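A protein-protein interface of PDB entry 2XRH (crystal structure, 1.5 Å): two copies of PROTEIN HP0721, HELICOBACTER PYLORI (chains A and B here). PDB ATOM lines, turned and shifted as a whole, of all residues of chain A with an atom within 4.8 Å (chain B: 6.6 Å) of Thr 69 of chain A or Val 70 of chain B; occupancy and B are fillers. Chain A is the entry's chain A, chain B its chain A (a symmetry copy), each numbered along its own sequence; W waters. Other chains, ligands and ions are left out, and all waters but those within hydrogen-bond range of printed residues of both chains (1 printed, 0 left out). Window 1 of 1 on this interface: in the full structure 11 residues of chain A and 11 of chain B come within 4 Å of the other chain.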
ATOM      1  N   THR A  65       0.949  20.327  24.433  1.00  0.00           N
ATOM      2  CA  THR A  65       0.592  18.945  24.796  1.00  0.00           C
ATOM      3  C   THR A  65      -0.909  18.671  24.886  1.00  0.00           C
ATOM      4  O   THR A  65      -1.288  17.493  24.970  1.00  0.00           O
ATOM      5  CB  THR A  65       1.292  18.509  26.118  1.00  0.00           C
ATOM      6  OG1 THR A  65       0.828  19.357  27.193  1.00  0.00           O
ATOM      7  CG2 THR A  65       2.804  18.573  25.964  1.00  0.00           C
ATOM      8  N   ASP A  66      -1.739  19.725  24.846  1.00  0.00           N
ATOM      9  CA  ASP A  66      -3.185  19.587  24.977  1.00  0.00           C
ATOM     10  C   ASP A  66      -3.809  18.553  24.054  1.00  0.00           C
ATOM     11  O   ASP A  66      -4.741  17.871  24.469  1.00  0.00           O
ATOM     12  CB  ASP A  66      -3.911  20.945  24.713  1.00  0.00           C
ATOM     13  CG  ASP A  66      -4.144  21.767  25.933  1.00  0.00           C
ATOM     14  OD1 ASP A  66      -4.016  21.268  27.073  1.00  0.00           O
ATOM     15  OD2 ASP A  66      -4.446  22.968  25.707  1.00  0.00           O
ATOM     16  N   LYS A  67      -3.347  18.473  22.805  1.00  0.00           N
ATOM     17  CA  LYS A  67      -3.948  17.591  21.771  1.00  0.00           C
ATOM     18  C   LYS A  67      -3.270  16.258  21.678  1.00  0.00           C
ATOM     19  O   LYS A  67      -3.702  15.417  20.887  1.00  0.00           O
ATOM     20  CB  LYS A  67      -3.910  18.312  20.418  1.00  0.00           C
ATOM     21  CG  LYS A  67      -4.649  19.660  20.471  1.00  0.00           C
ATOM     22  CD  LYS A  67      -5.958  19.712  21.329  1.00  0.00           C
ATOM     23  CE  LYS A  67      -6.713  21.095  21.339  1.00  0.00           C
ATOM     24  NZ  LYS A  67      -5.892  22.164  21.972  1.00  0.00           N
ATOM     25  N   MET A  68      -2.213  16.035  22.462  1.00  0.00           N
ATOM     26  CA  MET A  68      -1.579  14.717  22.479  1.00  0.00           C
ATOM     27  C   MET A  68      -2.550  13.746  23.133  1.00  0.00           C
ATOM     28  O   MET A  68      -3.382  14.144  23.945  1.00  0.00           O
ATOM     29  CB  MET A  68      -0.285  14.748  23.305  1.00  0.00           C
ATOM     30  CG  MET A  68       0.892  15.452  22.684  1.00  0.00           C
ATOM     31  SD  MET A  68       2.279  15.442  23.792  1.00  0.00           S
ATOM     32  CE  MET A  68       2.767  13.763  23.653  1.00  0.00           C
ATOM     33  N   THR A  69      -2.405  12.479  22.817  1.00  0.00           N
ATOM     34  CA  THR A  69      -3.126  11.448  23.578  1.00  0.00           C
ATOM     35  C   THR A  69      -2.460  11.276  24.940  1.00  0.00           C
ATOM     36  O   THR A  69      -1.280  11.492  25.116  1.00  0.00           O
ATOM     37  CB  THR A  69      -3.158  10.103  22.856  1.00  0.00           C
ATOM     38  OG1 THR A  69      -1.832   9.559  22.745  1.00  0.00           O
ATOM     39  CG2 THR A  69      -3.817  10.185  21.467  1.00  0.00           C
ATOM     40  N   VAL A  70      -3.253  10.845  25.918  1.00  0.00           N
ATOM     41  CA  VAL A  70      -2.712  10.506  27.214  1.00  0.00           C
ATOM     42  C   VAL A  70      -1.618   9.441  27.088  1.00  0.00           C
ATOM     43  O   VAL A  70      -0.595   9.527  27.755  1.00  0.00           O
ATOM     44  CB  VAL A  70      -3.807  10.062  28.157  1.00  0.00           C
ATOM     45  CG1 VAL A  70      -3.197   9.620  29.541  1.00  0.00           C
ATOM     46  CG2 VAL A  70      -4.785  11.210  28.338  1.00  0.00           C
ATOM     47  N   ALA A  71      -1.807   8.444  26.233  1.00  0.00           N
ATOM     48  CA  ALA A  71      -0.812   7.411  26.096  1.00  0.00           C
ATOM     49  C   ALA A  71       0.546   7.988  25.681  1.00  0.00           C
ATOM     50  O   ALA A  71       1.584   7.656  26.252  1.00  0.00           O
ATOM     51  CB  ALA A  71      -1.247   6.353  25.112  1.00  0.00           C
ATOM     52  N   ASP A  72       0.524   8.843  24.680  1.00  0.00           N
ATOM     53  CA  ASP A  72       1.762   9.412  24.175  1.00  0.00           C
ATOM     54  C   ASP A  72       2.340  10.386  25.221  1.00  0.00           C
ATOM     55  O   ASP A  72       3.551  10.444  25.397  1.00  0.00           O
ATOM     56  CB  ASP A  72       1.526  10.139  22.862  1.00  0.00           C
ATOM     57  CG  ASP A  72       1.283   9.221  21.703  1.00  0.00           C
ATOM     58  OD1 ASP A  72       1.755   8.072  21.715  1.00  0.00           O
ATOM     59  OD2 ASP A  72       0.601   9.676  20.771  1.00  0.00           O
ATOM     60  N   PHE A  73       1.486  11.163  25.892  1.00  0.00           N
ATOM     61  CA  PHE A  73       1.979  12.115  26.887  1.00  0.00           C
ATOM     62  C   PHE A  73       2.613  11.411  28.083  1.00  0.00           C
ATOM     63  O   PHE A  73       3.707  11.786  28.540  1.00  0.00           O
ATOM     64  CB  PHE A  73       0.865  13.032  27.351  1.00  0.00           C
ATOM     65  CG  PHE A  73       1.302  14.027  28.366  1.00  0.00           C
ATOM     66  CD1 PHE A  73       2.032  15.128  28.020  1.00  0.00           C
ATOM     67  CD2 PHE A  73       0.819  13.964  29.655  1.00  0.00           C
ATOM     68  CE1 PHE A  73       2.410  16.085  28.964  1.00  0.00           C
ATOM     69  CE2 PHE A  73       1.203  14.938  30.596  1.00  0.00           C
ATOM     70  CZ  PHE A  73       1.996  15.978  30.235  1.00  0.00           C
ATOM     71  N   PHE A  96       2.476  15.704  35.441  1.00  0.00           N
ATOM     72  CA  PHE A  96       2.085  16.426  34.189  1.00  0.00           C
ATOM     73  C   PHE A  96       3.183  17.410  33.760  1.00  0.00           C
ATOM     74  O   PHE A  96       2.995  18.174  32.803  1.00  0.00           O
ATOM     75  CB  PHE A  96       0.738  17.209  34.308  1.00  0.00           C
ATOM     76  CG  PHE A  96      -0.547  16.368  34.196  1.00  0.00           C
ATOM     77  CD1 PHE A  96      -1.253  16.224  33.012  1.00  0.00           C
ATOM     78  CD2 PHE A  96      -1.168  15.859  35.359  1.00  0.00           C
ATOM     79  CE1 PHE A  96      -2.414  15.441  32.940  1.00  0.00           C
ATOM     80  CE2 PHE A  96      -2.365  15.110  35.299  1.00  0.00           C
ATOM     81  CZ  PHE A  96      -2.995  14.904  34.076  1.00  0.00           C
ATOM     82  N   ARG A  99       3.159  21.472  32.325  1.00  0.00           N
ATOM     83  CA  ARG A  99       1.796  21.955  32.072  1.00  0.00           C
ATOM     84  C   ARG A  99       1.252  22.648  33.260  1.00  0.00           C
ATOM     85  O   ARG A  99       0.616  23.669  33.085  1.00  0.00           O
ATOM     86  CB  ARG A  99       0.776  20.854  31.713  1.00  0.00           C
ATOM     87  CG  ARG A  99       1.050  20.071  30.597  1.00  0.00           C
ATOM     88  CD  ARG A  99      -0.019  18.982  30.408  1.00  0.00           C
ATOM     89  NE  ARG A  99      -1.406  19.478  30.512  1.00  0.00           N
ATOM     90  CZ  ARG A  99      -2.146  19.951  29.522  1.00  0.00           C
ATOM     91  NH1 ARG A  99      -1.696  20.014  28.293  1.00  0.00           N
ATOM     92  NH2 ARG A  99      -3.383  20.363  29.757  1.00  0.00           N
ATOM     93  N   THR B  65      -8.455   5.567  29.167  1.00  0.00           N
ATOM     94  CA  THR B  65      -8.002   6.962  29.035  1.00  0.00           C
ATOM     95  C   THR B  65      -6.885   7.182  28.015  1.00  0.00           C
ATOM     96  O   THR B  65      -6.605   8.347  27.692  1.00  0.00           O
ATOM     97  CB  THR B  65      -7.586   7.553  30.416  1.00  0.00           C
ATOM     98  OG1 THR B  65      -6.466   6.797  30.928  1.00  0.00           O
ATOM     99  CG2 THR B  65      -8.763   7.536  31.378  1.00  0.00           C
ATOM    100  N   ASP B  66      -6.282   6.097  27.506  1.00  0.00           N
ATOM    101  CA  ASP B  66      -5.170   6.189  26.567  1.00  0.00           C
ATOM    102  C   ASP B  66      -5.420   7.101  25.377  1.00  0.00           C
ATOM    103  O   ASP B  66      -4.494   7.782  24.947  1.00  0.00           O
ATOM    104  CB  ASP B  66      -4.786   4.783  26.004  1.00  0.00           C
ATOM    105  CG  ASP B  66      -3.729   4.075  26.777  1.00  0.00           C
ATOM    106  OD1 ASP B  66      -3.038   4.688  27.620  1.00  0.00           O
ATOM    107  OD2 ASP B  66      -3.625   2.847  26.524  1.00  0.00           O
ATOM    108  N   LYS B  67      -6.630   7.077  24.816  1.00  0.00           N
ATOM    109  CA  LYS B  67      -6.967   7.829  23.579  1.00  0.00           C
ATOM    110  C   LYS B  67      -7.567   9.173  23.860  1.00  0.00           C
ATOM    111  O   LYS B  67      -7.852   9.914  22.918  1.00  0.00           O
ATOM    112  CB  LYS B  67      -7.917   6.981  22.724  1.00  0.00           C
ATOM    113  CG  LYS B  67      -7.301   5.616  22.373  1.00  0.00           C
ATOM    114  CD  LYS B  67      -5.767   5.595  22.061  1.00  0.00           C
ATOM    115  CE  LYS B  67      -5.169   4.190  21.672  1.00  0.00           C
ATOM    116  NZ  LYS B  67      -5.262   3.223  22.800  1.00  0.00           N
ATOM    117  N   MET B  68      -7.773   9.514  25.134  1.00  0.00           N
ATOM    118  CA  MET B  68      -8.264  10.851  25.464  1.00  0.00           C
ATOM    119  C   MET B  68      -7.155  11.842  25.146  1.00  0.00           C
ATOM    120  O   MET B  68      -5.978  11.492  25.170  1.00  0.00           O
ATOM    121  CB  MET B  68      -8.600  10.954  26.959  1.00  0.00           C
ATOM    122  CG  MET B  68      -9.843  10.241  27.419  1.00  0.00           C
ATOM    123  SD  MET B  68     -10.047  10.415  29.174  1.00  0.00           S
ATOM    124  CE  MET B  68     -10.559  12.091  29.255  1.00  0.00           C
ATOM    125  N   THR B  69      -7.531  13.077  24.901  1.00  0.00           N
ATOM    126  CA  THR B  69      -6.526  14.148  24.828  1.00  0.00           C
ATOM    127  C   THR B  69      -6.047  14.479  26.238  1.00  0.00           C
ATOM    128  O   THR B  69      -6.751  14.329  27.214  1.00  0.00           O
ATOM    129  CB  THR B  69      -7.066  15.413  24.166  1.00  0.00           C
ATOM    130  OG1 THR B  69      -8.106  15.997  24.967  1.00  0.00           O
ATOM    131  CG2 THR B  69      -7.573  15.169  22.733  1.00  0.00           C
ATOM    132  N   VAL B  70      -4.813  14.971  26.326  1.00  0.00           N
ATOM    133  CA  VAL B  70      -4.298  15.457  27.585  1.00  0.00           C
ATOM    134  C   VAL B  70      -5.206  16.548  28.163  1.00  0.00           C
ATOM    135  O   VAL B  70      -5.459  16.568  29.360  1.00  0.00           O
ATOM    136  CB  VAL B  70      -2.876  15.946  27.435  1.00  0.00           C
ATOM    137  CG1 VAL B  70      -2.352  16.545  28.794  1.00  0.00           C
ATOM    138  CG2 VAL B  70      -2.009  14.783  26.986  1.00  0.00           C
ATOM    139  N   ALA B  71      -5.714  17.448  27.330  1.00  0.00           N
ATOM    140  CA  ALA B  71      -6.557  18.502  27.833  1.00  0.00           C
ATOM    141  C   ALA B  71      -7.790  17.943  28.554  1.00  0.00           C
ATOM    142  O   ALA B  71      -8.137  18.370  29.654  1.00  0.00           O
ATOM    143  CB  ALA B  71      -6.985  19.440  26.731  1.00  0.00           C
ATOM    144  N   ASP B  72      -8.444  16.993  27.918  1.00  0.00           N
ATOM    145  CA  ASP B  72      -9.654  16.428  28.489  1.00  0.00           C
ATOM    146  C   ASP B  72      -9.289  15.585  29.727  1.00  0.00           C
ATOM    147  O   ASP B  72     -10.021  15.593  30.710  1.00  0.00           O
ATOM    148  CB  ASP B  72     -10.382  15.567  27.471  1.00  0.00           C
ATOM    149  CG  ASP B  72     -11.062  16.357  26.395  1.00  0.00           C
ATOM    150  OD1 ASP B  72     -11.435  17.519  26.623  1.00  0.00           O
ATOM    151  OD2 ASP B  72     -11.216  15.786  25.304  1.00  0.00           O
ATOM    152  N   PHE B  73      -8.179  14.844  29.674  1.00  0.00           N
ATOM    153  CA  PHE B  73      -7.789  14.014  30.814  1.00  0.00           C
ATOM    154  C   PHE B  73      -7.426  14.857  32.033  1.00  0.00           C
ATOM    155  O   PHE B  73      -7.865  14.573  33.162  1.00  0.00           O
ATOM    156  CB  PHE B  73      -6.636  13.102  30.447  1.00  0.00           C
ATOM    157  CG  PHE B  73      -6.191  12.230  31.565  1.00  0.00           C
ATOM    158  CD1 PHE B  73      -6.908  11.131  31.943  1.00  0.00           C
ATOM    159  CD2 PHE B  73      -4.945  12.400  32.126  1.00  0.00           C
ATOM    160  CE1 PHE B  73      -6.473  10.287  32.968  1.00  0.00           C
ATOM    161  CE2 PHE B  73      -4.514  11.539  33.154  1.00  0.00           C
ATOM    162  CZ  PHE B  73      -5.289  10.502  33.560  1.00  0.00           C
ATOM    163  N   GLU B  74      -6.666  15.910  31.814  1.00  0.00           N
ATOM    164  CA  GLU B  74      -6.295  16.797  32.895  1.00  0.00           C
ATOM    165  C   GLU B  74      -7.516  17.475  33.518  1.00  0.00           C
ATOM    166  O   GLU B  74      -7.624  17.615  34.750  1.00  0.00           O
ATOM    167  CB  GLU B  74      -5.319  17.855  32.418  1.00  0.00           C
ATOM    168  CG  GLU B  74      -4.764  18.679  33.532  1.00  0.00           C
ATOM    169  CD  GLU B  74      -3.838  19.709  33.011  1.00  0.00           C
ATOM    170  OE1 GLU B  74      -4.354  20.711  32.490  1.00  0.00           O
ATOM    171  OE2 GLU B  74      -2.607  19.493  33.087  1.00  0.00           O
ATOM    172  N   ALA B  75      -8.456  17.882  32.678  1.00  0.00           N
ATOM    173  CA  ALA B  75      -9.692  18.513  33.191  1.00  0.00           C
ATOM    174  C   ALA B  75     -10.396  17.547  34.113  1.00  0.00           C
ATOM    175  O   ALA B  75     -10.846  17.940  35.188  1.00  0.00           O
ATOM    176  CB  ALA B  75     -10.647  18.939  32.040  1.00  0.00           C
HETATM  177  O   HOH W   1      -2.676  23.048  32.095  1.00  0.00           O
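The backbone carbonyl oxygen of Met 68 of chain A is in hydrogen-bond range of the backbone NH of Val 70 of chain B, at 2.9 Å. The backbone carbonyl oxygen (O) of Asp 66 of chain A sits at hydrogen-bond distance from the backbone NH (N) of Ala 71 of chain B. N of Val 70 of chain A lies within hydrogen-bond range of O of Met 68 of chain B, 2.9 Å away. The backbone NH of Ala 71 of chain A is in hydrogen-bond range of the backbone carbonyl oxygen of Asp 66 of chain B (3.1 Å). The backbone NH of Val 70 of chain A is in hydrogen-bond range of the backbone carbonyl oxygen of Asp 66 of chain B, at 3.4 Å. N of Val 70 of chain B is in hydrogen-bond range of O of Asp 66 of chain A (3.4 Å). The side-chain carboxylate of Glu 74 of chain B lies within salt-bridge range of the guanidinium group of Arg 99 of chain A (2.8 Å).
Asp 66 of chain A touches Val 70 of chain B, and with the chains exchanged Val 70 of chain A touches Asp 66 of chain B. Met 68 of chain A touches its own counterpart, Met 68 of chain B. Met 68 of chain A touches Thr 69 of chain B, and with the chains exchanged Thr 69 of chain A touches Met 68 of chain B. Val 70 of chain A touches Phe 73 of chain B, and with the chains exchanged Phe 73 of chain A touches Val 70 of chain B.
Thr 69 of chain A touches just these residues of chain B: Asp 66 (3.4 Å), Met 68 (3.3 Å) and Val 70 (3.9 Å). Of the printed residues of chain B, Asp 66 of chain A touches Thr 69, Val 70 and Ala 71. Of the printed residues of chain B, Arg 99 of chain A touches Val 70 and Glu 74. Of the printed residues of chain A, Glu 74 of chain B touches Phe 96 (3.5 Å) and Arg 99 (2.8 Å). Of the printed residues of chain B, Thr 65 of chain A touches Val 70 (3.3 Å). Lys 67 of chain A touches none of the printed residues of chain B. The nearest residue of chain B that does not touch Thr 69 of chain A is Lys 67 of chain B (4.3 Å). The nearest printed residue of chain B that does not touch Thr 65 of chain A is Ala 71 of chain B (5.0 Å).
Water W1 lies within hydrogen-bond range of OE1 of Glu 74 of chain B (2.9 Å) and O of Arg 99 of chain A (3.5 Å).
Val 70 of chain B touches Thr 65 of chain A. CB of Thr 69 of chain B touches O of Asp 66 of chain A, 3.4 Å away. Met 68 of chain A touches Met 68 of chain B (O to O, 3.9 Å). Met 68 of chain A touches Thr 69 of chain B. Asp 66 of chain B touches Thr 69 of chain A. O of Thr 69 of chain A touches CG2 of Val 70 of chain B, 3.9 Å away. CB of Val 70 of chain A touches O of Thr 65 of chain B, 3.3 Å away. Phe 73 of chain A touches Val 70 of chain B. Glu 74 of chain B touches Phe 96 of chain A. Val 70 of chain B touches Arg 99 of chain A.
Of the 11 printed residues of chain A, 9 touch a printed residue of chain B. Printed residues of chain A that touch a printed residue of chain B: Thr 65, Asp 66, Met 68, Thr 69, Val 70, Ala 71, Phe 73, Phe 96 and Arg 99. Hydrophobic or aromatic side chains of chain A that line the printed part of chain B: Val 70, Ala 71, Phe 73 and Phe 96. Of the 11 printed residues of chain B, 8 touch a printed residue of chain A. Hydrophobic or aromatic side chains of chain B that line the printed part of chain A: Val 70, Ala 71 and Phe 73. Among the printed residues, Asp or Glu carboxylates within 4 Å of a Lys or Arg side-chain nitrogen of the other chain: Arg 99 of chain A with Glu 74 of chain B.
The side-chain hydroxyl of Thr 65 of chain A sits at hydrogen-bond distance from the guanidinium group of Arg 99 of chain A, at 2.8 Å. The guanidinium group (NH2) of Arg 99 of chain A lies within salt-bridge range of the side-chain carboxylate (OD1) of Asp 66 of chain A. OG1 of Thr 69 of chain A lies within hydrogen-bond range of N of Asp 72 of chain A (3.1 Å). OG1 of Thr 69 of chain B is in hydrogen-bond range of N of Asp 72 of chain B, at 3.1 Å.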
